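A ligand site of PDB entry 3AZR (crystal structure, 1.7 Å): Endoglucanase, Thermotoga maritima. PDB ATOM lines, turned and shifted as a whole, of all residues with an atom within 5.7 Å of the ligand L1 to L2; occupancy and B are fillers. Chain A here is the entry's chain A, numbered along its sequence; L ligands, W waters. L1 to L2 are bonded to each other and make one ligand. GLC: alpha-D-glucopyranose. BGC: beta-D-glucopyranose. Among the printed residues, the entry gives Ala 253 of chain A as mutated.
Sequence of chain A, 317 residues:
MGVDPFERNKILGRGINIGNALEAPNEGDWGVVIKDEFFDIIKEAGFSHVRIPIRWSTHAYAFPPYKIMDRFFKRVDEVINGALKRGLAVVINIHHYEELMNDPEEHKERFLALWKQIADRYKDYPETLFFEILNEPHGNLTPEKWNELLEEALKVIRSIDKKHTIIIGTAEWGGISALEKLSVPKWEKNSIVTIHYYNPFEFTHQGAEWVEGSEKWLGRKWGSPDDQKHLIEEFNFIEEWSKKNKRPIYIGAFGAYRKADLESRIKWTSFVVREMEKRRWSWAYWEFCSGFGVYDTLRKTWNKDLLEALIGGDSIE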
ATOM      1  N   ASN A  20      22.193 -12.324   6.335  1.00  0.00           N
ATOM      2  CA  ASN A  20      21.004 -13.032   5.866  1.00  0.00           C
ATOM      3  C   ASN A  20      21.428 -14.017   4.772  1.00  0.00           C
ATOM      4  O   ASN A  20      20.696 -14.317   3.848  1.00  0.00           O
ATOM      5  CB  ASN A  20      19.902 -12.061   5.387  1.00  0.00           C
ATOM      6  CG  ASN A  20      19.001 -11.600   6.540  1.00  0.00           C
ATOM      7  OD1 ASN A  20      18.023 -10.888   6.348  1.00  0.00           O
ATOM      8  ND2 ASN A  20      19.313 -12.051   7.754  1.00  0.00           N
ATOM      9  N   GLU A  23      24.407 -17.413   7.674  1.00  0.00           N
ATOM     10  CA  GLU A  23      23.991 -17.592   9.061  1.00  0.00           C
ATOM     11  C   GLU A  23      22.513 -18.041   9.189  1.00  0.00           C
ATOM     12  O   GLU A  23      22.015 -18.331  10.258  1.00  0.00           O
ATOM     13  CB  GLU A  23      24.358 -16.336   9.916  1.00  0.00           C
ATOM     14  CG  GLU A  23      23.329 -15.223   9.932  1.00  0.00           C
ATOM     15  CD  GLU A  23      23.375 -14.396   8.671  1.00  0.00           C
ATOM     16  OE1 GLU A  23      23.877 -14.870   7.632  1.00  0.00           O
ATOM     17  OE2 GLU A  23      22.907 -13.225   8.734  1.00  0.00           O
ATOM     18  N   TRP A  30      17.153 -16.854   4.115  1.00  0.00           N
ATOM     19  CA  TRP A  30      16.828 -15.534   4.594  1.00  0.00           C
ATOM     20  C   TRP A  30      16.978 -14.469   3.495  1.00  0.00           C
ATOM     21  O   TRP A  30      17.087 -13.300   3.781  1.00  0.00           O
ATOM     22  CB  TRP A  30      17.678 -15.204   5.817  1.00  0.00           C
ATOM     23  CG  TRP A  30      17.262 -16.019   7.057  1.00  0.00           C
ATOM     24  CD1 TRP A  30      16.262 -16.997   7.151  1.00  0.00           C
ATOM     25  CD2 TRP A  30      17.876 -15.986   8.344  1.00  0.00           C
ATOM     26  NE1 TRP A  30      16.254 -17.551   8.409  1.00  0.00           N
ATOM     27  CE2 TRP A  30      17.225 -16.951   9.158  1.00  0.00           C
ATOM     28  CE3 TRP A  30      18.930 -15.225   8.893  1.00  0.00           C
ATOM     29  CZ2 TRP A  30      17.581 -17.164  10.497  1.00  0.00           C
ATOM     30  CZ3 TRP A  30      19.282 -15.446  10.204  1.00  0.00           C
ATOM     31  CH2 TRP A  30      18.606 -16.402  11.001  1.00  0.00           C
ATOM     32  N   ARG A  51      32.630  -8.994   6.376  1.00  0.00           N
ATOM     33  CA  ARG A  51      32.388  -9.863   7.518  1.00  0.00           C
ATOM     34  C   ARG A  51      31.355 -10.883   7.072  1.00  0.00           C
ATOM     35  O   ARG A  51      30.302 -10.530   6.474  1.00  0.00           O
ATOM     36  CB  ARG A  51      31.900  -9.082   8.744  1.00  0.00           C
ATOM     37  CG  ARG A  51      31.580  -9.969   9.966  1.00  0.00           C
ATOM     38  CD  ARG A  51      31.522  -9.074  11.291  1.00  0.00           C
ATOM     39  NE  ARG A  51      31.142  -9.910  12.463  1.00  0.00           N
ATOM     40  CZ  ARG A  51      29.896 -10.141  12.850  1.00  0.00           C
ATOM     41  NH1 ARG A  51      28.857  -9.633  12.173  1.00  0.00           N
ATOM     42  NH2 ARG A  51      29.651 -10.814  13.964  1.00  0.00           N
ATOM     43  N   HIS A  95      28.095 -18.015  14.206  1.00  0.00           N
ATOM     44  CA  HIS A  95      26.932 -17.176  14.342  1.00  0.00           C
ATOM     45  C   HIS A  95      25.607 -18.038  14.536  1.00  0.00           C
ATOM     46  O   HIS A  95      25.513 -18.990  14.010  1.00  0.00           O
ATOM     47  CB  HIS A  95      26.820 -16.336  13.088  1.00  0.00           C
ATOM     48  CG  HIS A  95      26.143 -14.970  13.203  1.00  0.00           C
ATOM     49  ND1 HIS A  95      26.784 -13.789  12.963  1.00  0.00           N
ATOM     50  CD2 HIS A  95      24.862 -14.651  13.409  1.00  0.00           C
ATOM     51  CE1 HIS A  95      25.911 -12.798  13.052  1.00  0.00           C
ATOM     52  NE2 HIS A  95      24.749 -13.303  13.288  1.00  0.00           N
ATOM     53  N   HIS A  96      24.714 -17.517  15.382  1.00  0.00           N
ATOM     54  CA  HIS A  96      23.470 -18.223  15.682  1.00  0.00           C
ATOM     55  C   HIS A  96      23.645 -19.665  16.147  1.00  0.00           C
ATOM     56  O   HIS A  96      22.953 -20.573  15.660  1.00  0.00           O
ATOM     57  CB  HIS A  96      22.481 -18.155  14.485  1.00  0.00           C
ATOM     58  CG  HIS A  96      21.990 -16.758  14.232  1.00  0.00           C
ATOM     59  ND1 HIS A  96      21.795 -16.237  12.964  1.00  0.00           N
ATOM     60  CD2 HIS A  96      21.701 -15.769  15.097  1.00  0.00           C
ATOM     61  CE1 HIS A  96      21.424 -14.978  13.070  1.00  0.00           C
ATOM     62  NE2 HIS A  96      21.351 -14.658  14.350  1.00  0.00           N
ATOM     63  N   ASN A 135      29.567 -14.782  17.709  1.00  0.00           N
ATOM     64  CA  ASN A 135      28.684 -13.626  17.550  1.00  0.00           C
ATOM     65  C   ASN A 135      27.693 -13.531  18.695  1.00  0.00           C
ATOM     66  O   ASN A 135      27.003 -14.487  19.003  1.00  0.00           O
ATOM     67  CB  ASN A 135      27.844 -13.788  16.288  1.00  0.00           C
ATOM     68  CG  ASN A 135      26.903 -12.618  16.043  1.00  0.00           C
ATOM     69  OD1 ASN A 135      27.357 -11.529  15.733  1.00  0.00           O
ATOM     70  ND2 ASN A 135      25.600 -12.863  16.160  1.00  0.00           N
ATOM     71  N   GLU A 136      27.626 -12.341  19.273  1.00  0.00           N
ATOM     72  CA  GLU A 136      26.674 -11.995  20.346  1.00  0.00           C
ATOM     73  C   GLU A 136      26.295 -13.003  21.436  1.00  0.00           C
ATOM     74  O   GLU A 136      25.156 -13.470  21.494  1.00  0.00           O
ATOM     75  CB  GLU A 136      25.401 -11.452  19.681  1.00  0.00           C
ATOM     76  CG  GLU A 136      25.700 -10.214  18.825  1.00  0.00           C
ATOM     77  CD  GLU A 136      24.473  -9.518  18.209  1.00  0.00           C
ATOM     78  OE1 GLU A 136      23.332 -10.009  18.310  1.00  0.00           O
ATOM     79  OE2 GLU A 136      24.665  -8.447  17.608  1.00  0.00           O
ATOM     80  N   HIS A 196      28.859  -4.447  18.769  1.00  0.00           N
ATOM     81  CA  HIS A 196      27.836  -4.132  17.792  1.00  0.00           C
ATOM     82  C   HIS A 196      27.095  -2.903  18.341  1.00  0.00           C
ATOM     83  O   HIS A 196      26.864  -2.803  19.554  1.00  0.00           O
ATOM     84  CB  HIS A 196      26.934  -5.373  17.606  1.00  0.00           C
ATOM     85  CG  HIS A 196      27.705  -6.552  17.089  1.00  0.00           C
ATOM     86  ND1 HIS A 196      27.198  -7.838  17.026  1.00  0.00           N
ATOM     87  CD2 HIS A 196      28.975  -6.616  16.617  1.00  0.00           C
ATOM     88  CE1 HIS A 196      28.118  -8.632  16.522  1.00  0.00           C
ATOM     89  NE2 HIS A 196      29.199  -7.917  16.258  1.00  0.00           N
ATOM     90  N   TYR A 198      23.704  -0.567  17.889  1.00  0.00           N
ATOM     91  CA  TYR A 198      22.414  -0.373  17.265  1.00  0.00           C
ATOM     92  C   TYR A 198      21.596   0.588  18.088  1.00  0.00           C
ATOM     93  O   TYR A 198      20.380   0.614  17.967  1.00  0.00           O
ATOM     94  CB  TYR A 198      21.714  -1.718  17.196  1.00  0.00           C
ATOM     95  CG  TYR A 198      22.313  -2.655  16.171  1.00  0.00           C
ATOM     96  CD1 TYR A 198      22.119  -2.430  14.821  1.00  0.00           C
ATOM     97  CD2 TYR A 198      22.979  -3.806  16.547  1.00  0.00           C
ATOM     98  CE1 TYR A 198      22.526  -3.335  13.854  1.00  0.00           C
ATOM     99  CE2 TYR A 198      23.411  -4.729  15.592  1.00  0.00           C
ATOM    100  CZ  TYR A 198      23.172  -4.489  14.258  1.00  0.00           C
ATOM    101  OH  TYR A 198      23.549  -5.431  13.322  1.00  0.00           O
ATOM    102  N   HIS A 205      15.839  -0.789  15.159  1.00  0.00           N
ATOM    103  CA  HIS A 205      15.056  -1.982  15.129  1.00  0.00           C
ATOM    104  C   HIS A 205      13.558  -1.821  15.028  1.00  0.00           C
ATOM    105  O   HIS A 205      12.832  -2.714  15.134  1.00  0.00           O
ATOM    106  CB  HIS A 205      15.511  -2.944  16.251  1.00  0.00           C
ATOM    107  CG  HIS A 205      16.801  -3.652  15.989  1.00  0.00           C
ATOM    108  ND1 HIS A 205      18.012  -3.061  15.971  1.00  0.00           N
ATOM    109  CD2 HIS A 205      17.014  -4.932  15.719  1.00  0.00           C
ATOM    110  CE1 HIS A 205      18.924  -3.954  15.697  1.00  0.00           C
ATOM    111  NE2 HIS A 205      18.331  -5.084  15.495  1.00  0.00           N
ATOM    112  N   TRP A 210      11.602  -9.825  13.801  1.00  0.00           N
ATOM    113  CA  TRP A 210      12.156 -10.826  14.713  1.00  0.00           C
ATOM    114  C   TRP A 210      12.358 -10.309  16.136  1.00  0.00           C
ATOM    115  O   TRP A 210      12.925 -11.013  16.979  1.00  0.00           O
ATOM    116  CB  TRP A 210      13.495 -11.363  14.145  1.00  0.00           C
ATOM    117  CG  TRP A 210      14.574 -10.322  13.995  1.00  0.00           C
ATOM    118  CD1 TRP A 210      15.585 -10.057  14.860  1.00  0.00           C
ATOM    119  CD2 TRP A 210      14.672  -9.322  12.957  1.00  0.00           C
ATOM    120  NE1 TRP A 210      16.313  -8.966  14.444  1.00  0.00           N
ATOM    121  CE2 TRP A 210      15.760  -8.481  13.287  1.00  0.00           C
ATOM    122  CE3 TRP A 210      13.943  -9.058  11.802  1.00  0.00           C
ATOM    123  CZ2 TRP A 210      16.141  -7.383  12.496  1.00  0.00           C
ATOM    124  CZ3 TRP A 210      14.321  -7.976  11.019  1.00  0.00           C
ATOM    125  CH2 TRP A 210      15.412  -7.145  11.369  1.00  0.00           C
ATOM    126  N   VAL A 211      11.907  -9.089  16.407  1.00  0.00           N
ATOM    127  CA  VAL A 211      12.049  -8.522  17.740  1.00  0.00           C
ATOM    128  C   VAL A 211      10.695  -8.264  18.344  1.00  0.00           C
ATOM    129  O   VAL A 211       9.902  -7.484  17.820  1.00  0.00           O
ATOM    130  CB  VAL A 211      12.846  -7.209  17.714  1.00  0.00           C
ATOM    131  CG1 VAL A 211      12.946  -6.633  19.140  1.00  0.00           C
ATOM    132  CG2 VAL A 211      14.225  -7.476  17.126  1.00  0.00           C
ATOM    133  N   ALA A 253      29.199  -4.727  13.621  1.00  0.00           N
ATOM    134  CA  ALA A 253      27.854  -4.649  13.046  1.00  0.00           C
ATOM    135  C   ALA A 253      27.143  -3.399  13.596  1.00  0.00           C
ATOM    136  O   ALA A 253      27.187  -3.152  14.814  1.00  0.00           O
ATOM    137  CB  ALA A 253      27.034  -5.904  13.373  1.00  0.00           C
ATOM    138  N   TRP A 286      25.988  -3.287   8.892  1.00  0.00           N
ATOM    139  CA  TRP A 286      24.996  -4.367   8.813  1.00  0.00           C
ATOM    140  C   TRP A 286      23.820  -3.751   8.027  1.00  0.00           C
ATOM    141  O   TRP A 286      23.147  -2.876   8.575  1.00  0.00           O
ATOM    142  CB  TRP A 286      24.491  -4.772  10.185  1.00  0.00           C
ATOM    143  CG  TRP A 286      23.545  -5.965  10.145  1.00  0.00           C
ATOM    144  CD1 TRP A 286      22.177  -5.956  10.065  1.00  0.00           C
ATOM    145  CD2 TRP A 286      23.949  -7.327  10.082  1.00  0.00           C
ATOM    146  NE1 TRP A 286      21.687  -7.257   9.965  1.00  0.00           N
ATOM    147  CE2 TRP A 286      22.765  -8.114   9.955  1.00  0.00           C
ATOM    148  CE3 TRP A 286      25.189  -7.970  10.104  1.00  0.00           C
ATOM    149  CZ2 TRP A 286      22.796  -9.515   9.860  1.00  0.00           C
ATOM    150  CZ3 TRP A 286      25.215  -9.349  10.012  1.00  0.00           C
ATOM    151  CH2 TRP A 286      24.041 -10.107   9.894  1.00  0.00           C
ATOM    152  N   GLU A 287      23.573  -4.174   6.790  1.00  0.00           N
ATOM    153  CA  GLU A 287      24.360  -5.170   6.056  1.00  0.00           C
ATOM    154  C   GLU A 287      24.309  -4.882   4.557  1.00  0.00           C
ATOM    155  O   GLU A 287      23.684  -3.888   4.131  1.00  0.00           O
ATOM    156  CB  GLU A 287      23.954  -6.612   6.409  1.00  0.00           C
ATOM    157  CG  GLU A 287      22.491  -6.869   6.730  1.00  0.00           C
ATOM    158  CD  GLU A 287      21.562  -6.687   5.549  1.00  0.00           C
ATOM    159  OE1 GLU A 287      21.994  -6.847   4.393  1.00  0.00           O
ATOM    160  OE2 GLU A 287      20.370  -6.389   5.769  1.00  0.00           O
ATOM    161  N   SER A 290      20.202  -6.834   2.200  1.00  0.00           N
ATOM    162  CA  SER A 290      18.934  -7.384   2.634  1.00  0.00           C
ATOM    163  C   SER A 290      18.106  -6.297   3.326  1.00  0.00           C
ATOM    164  O   SER A 290      18.115  -5.153   2.857  1.00  0.00           O
ATOM    165  CB  SER A 290      19.197  -8.627   3.529  1.00  0.00           C
ATOM    166  OG  SER A 290      18.022  -9.201   4.002  1.00  0.00           O
ATOM    167  N   PHE A 292      18.553  -4.405   5.837  1.00  0.00           N
ATOM    168  CA  PHE A 292      19.295  -3.227   6.281  1.00  0.00           C
ATOM    169  C   PHE A 292      20.189  -2.815   5.106  1.00  0.00           C
ATOM    170  O   PHE A 292      21.060  -1.969   5.249  1.00  0.00           O
ATOM    171  CB  PHE A 292      20.237  -3.562   7.450  1.00  0.00           C
ATOM    172  CG  PHE A 292      19.566  -3.764   8.789  1.00  0.00           C
ATOM    173  CD1 PHE A 292      19.739  -2.815   9.808  1.00  0.00           C
ATOM    174  CD2 PHE A 292      18.874  -4.940   9.086  1.00  0.00           C
ATOM    175  CE1 PHE A 292      19.257  -3.046  11.106  1.00  0.00           C
ATOM    176  CE2 PHE A 292      18.371  -5.180  10.382  1.00  0.00           C
ATOM    177  CZ  PHE A 292      18.565  -4.231  11.398  1.00  0.00           C
HETATM  178  C1  GLC L   1      23.054  -8.417  15.031  1.00  0.00           C
HETATM  179  C2  GLC L   1      22.905  -9.934  14.847  1.00  0.00           C
HETATM  180  C3  GLC L   1      22.366 -10.215  13.446  1.00  0.00           C
HETATM  181  C4  GLC L   1      21.033  -9.500  13.272  1.00  0.00           C
HETATM  182  C5  GLC L   1      21.304  -8.013  13.441  1.00  0.00           C
HETATM  183  C6  GLC L   1      19.994  -7.218  13.265  1.00  0.00           C
HETATM  184  O1  GLC L   1      24.072  -7.909  14.159  1.00  0.00           O
HETATM  185  O2  GLC L   1      24.191 -10.536  14.981  1.00  0.00           O
HETATM  186  O3  GLC L   1      22.191 -11.624  13.231  1.00  0.00           O
HETATM  187  O4  GLC L   1      20.551  -9.713  11.934  1.00  0.00           O
HETATM  188  O5  GLC L   1      21.817  -7.744  14.758  1.00  0.00           O
HETATM  189  O6  GLC L   1      19.126  -7.511  14.362  1.00  0.00           O
HETATM  190  C2  BGC L   2      18.705  -9.905  10.450  1.00  0.00           C
HETATM  191  C3  BGC L   2      17.242 -10.340  10.337  1.00  0.00           C
HETATM  192  C4  BGC L   2      17.108 -11.768  10.859  1.00  0.00           C
HETATM  193  C5  BGC L   2      17.682 -11.850  12.280  1.00  0.00           C
HETATM  194  C6  BGC L   2      17.569 -13.286  12.794  1.00  0.00           C
HETATM  195  C1  BGC L   2      19.173 -10.066  11.897  1.00  0.00           C
HETATM  196  O2  BGC L   2      18.926  -8.557  10.009  1.00  0.00           O
HETATM  197  O3  BGC L   2      16.837 -10.356   8.964  1.00  0.00           O
HETATM  198  O4  BGC L   2      15.727 -12.144  10.866  1.00  0.00           O
HETATM  199  O5  BGC L   2      19.065 -11.450  12.270  1.00  0.00           O
HETATM  200  O6  BGC L   2      18.020 -13.323  14.157  1.00  0.00           O
HETATM  201  C2  BGC L   3      19.049  -8.910  18.197  1.00  0.00           C
HETATM  202  C3  BGC L   3      17.577  -9.024  18.591  1.00  0.00           C
HETATM  203  C4  BGC L   3      17.453  -9.045  20.112  1.00  0.00           C
HETATM  204  C5  BGC L   3      18.150  -7.819  20.702  1.00  0.00           C
HETATM  205  C6  BGC L   3      18.051  -7.868  22.230  1.00  0.00           C
HETATM  206  C1  BGC L   3      19.674  -7.687  18.884  1.00  0.00           C
HETATM  207  O1  BGC L   3      21.070  -7.602  18.549  1.00  0.00           O
HETATM  208  O2  BGC L   3      19.151  -8.769  16.774  1.00  0.00           O
HETATM  209  O3  BGC L   3      17.034 -10.232  18.042  1.00  0.00           O
HETATM  210  O4  BGC L   3      16.068  -9.040  20.488  1.00  0.00           O
HETATM  211  O5  BGC L   3      19.540  -7.811  20.301  1.00  0.00           O
HETATM  212  O6  BGC L   3      18.721  -6.728  22.794  1.00  0.00           O
HETATM  213  O   HOH W   1      18.911  -7.972   7.562  1.00  0.00           O
HETATM  214  O   HOH W   2      26.275  -9.462  13.593  1.00  0.00           O
HETATM  215  O   HOH W   3      21.356 -12.843  10.929  1.00  0.00           O
HETATM  216  O   HOH W   4      19.718 -11.845  15.960  1.00  0.00           O
HETATM  217  O   HOH W   5      16.096  -8.119   7.080  1.00  0.00           O
HETATM  218  O   HOH W   6      14.942 -14.488  10.573  1.00  0.00           O
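OH of Tyr 198 is in hydrogen-bond range of O1 of GLC L1.
NE2 of His 205 sits at hydrogen-bond distance from O6 of GLC L1 (2.8 Å).
The side-chain amide oxygen (OD1) of Asn 20 sits at hydrogen-bond distance from an oxygen (O3) of BGC L2 (2.9 Å).
ND2 of Asn 135 lies within hydrogen-bond range of O2 of GLC L1 (3.0 Å).
OE2 of Glu 136 sits close to O2 of GLC L1.
The indole nitrogen of Trp 286 is in hydrogen-bond range of an oxygen (O2) of BGC L2, 3.1 Å away.
An oxygen (O3) of GLC L1 sits at hydrogen-bond distance from a ring nitrogen (NE2) of His 95 (3.1 Å).
The indole nitrogen (NE1) of Trp 210 is in hydrogen-bond range of an oxygen (O6) of GLC L1 (3.2 Å).
NE2 of His 96 sits at hydrogen-bond distance from O3 of GLC L1.
The side-chain carboxylate (OE1) of Glu 136 sits at hydrogen-bond distance from an oxygen (O1) of BGC L3 (3.3 Å).
An oxygen (O6) of GLC L1 lies within hydrogen-bond range of an oxygen (O2) of BGC L3, 2.7 Å away.
OE2 of Glu 23 lies within hydrogen-bond range of N of Asn 20.
OG of Ser 290 sits at hydrogen-bond distance from OD1 of Asn 20, 2.9 Å away.
The side-chain amide nitrogen (ND2) of Asn 135 sits at hydrogen-bond distance from a ring nitrogen (NE2) of His 95, at 3.0 Å.
The guanidinium group (NH2) of Arg 51 lies within hydrogen-bond range of the side-chain amide oxygen (OD1) of Asn 135 (3.0 Å).
The side-chain carboxylate (OE2) of Glu 136 sits at hydrogen-bond distance from a ring nitrogen (ND1) of His 196 (2.7 Å).
O of Glu 23 sits at hydrogen-bond distance from ND1 of His 96 (3.4 Å).
N of Phe 292 is in hydrogen-bond range of OE2 of Glu 287 (2.7 Å).
Merely in contact with the ligand L1 to L2: Trp 30 (3.7 Å), Ala 253 (3.7 Å) and Phe 292 (3.4 Å).
Hydrophobic or aromatic side chains that line the ligand L1 to L2: Trp 30, His 95, His 96, Tyr 198, His 205, Trp 210, Ala 253, Trp 286 and Phe 292.
Of the 18 residues printed, 12 come within 4 Å of the ligand L1 to L2.
The nearest printed residue that does not touch the ligand L1 to L2 is His 196 (4.2 Å).
Water W1 lies within hydrogen-bond range of an oxygen (O2) of BGC L2 (2.5 Å), the side-chain carboxylate (OE2) of Glu 287 (2.8 Å) and the side-chain amide oxygen (OD1) of Asn 20 (3.3 Å).
Water W2 lies within hydrogen-bond range of an oxygen (O2) of GLC L1 (2.7 Å), the guanidinium group (NH1) of Arg 51 (3.0 Å) and the side-chain amide oxygen (OD1) of Asn 135 (3.2 Å).
Water W3 bridges the side-chain carboxylate of Glu 23 (2.7 Å) and an oxygen (O3) of GLC L1 (2.7 Å).
Water W4 lies within hydrogen-bond range of an oxygen (O6) of BGC L2 and an oxygen (O2) of BGC L3.
Water W5 bridges an oxygen (O3) of BGC L2 (3.0 Å) and the side-chain amide oxygen of Asn 20 (3.5 Å).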
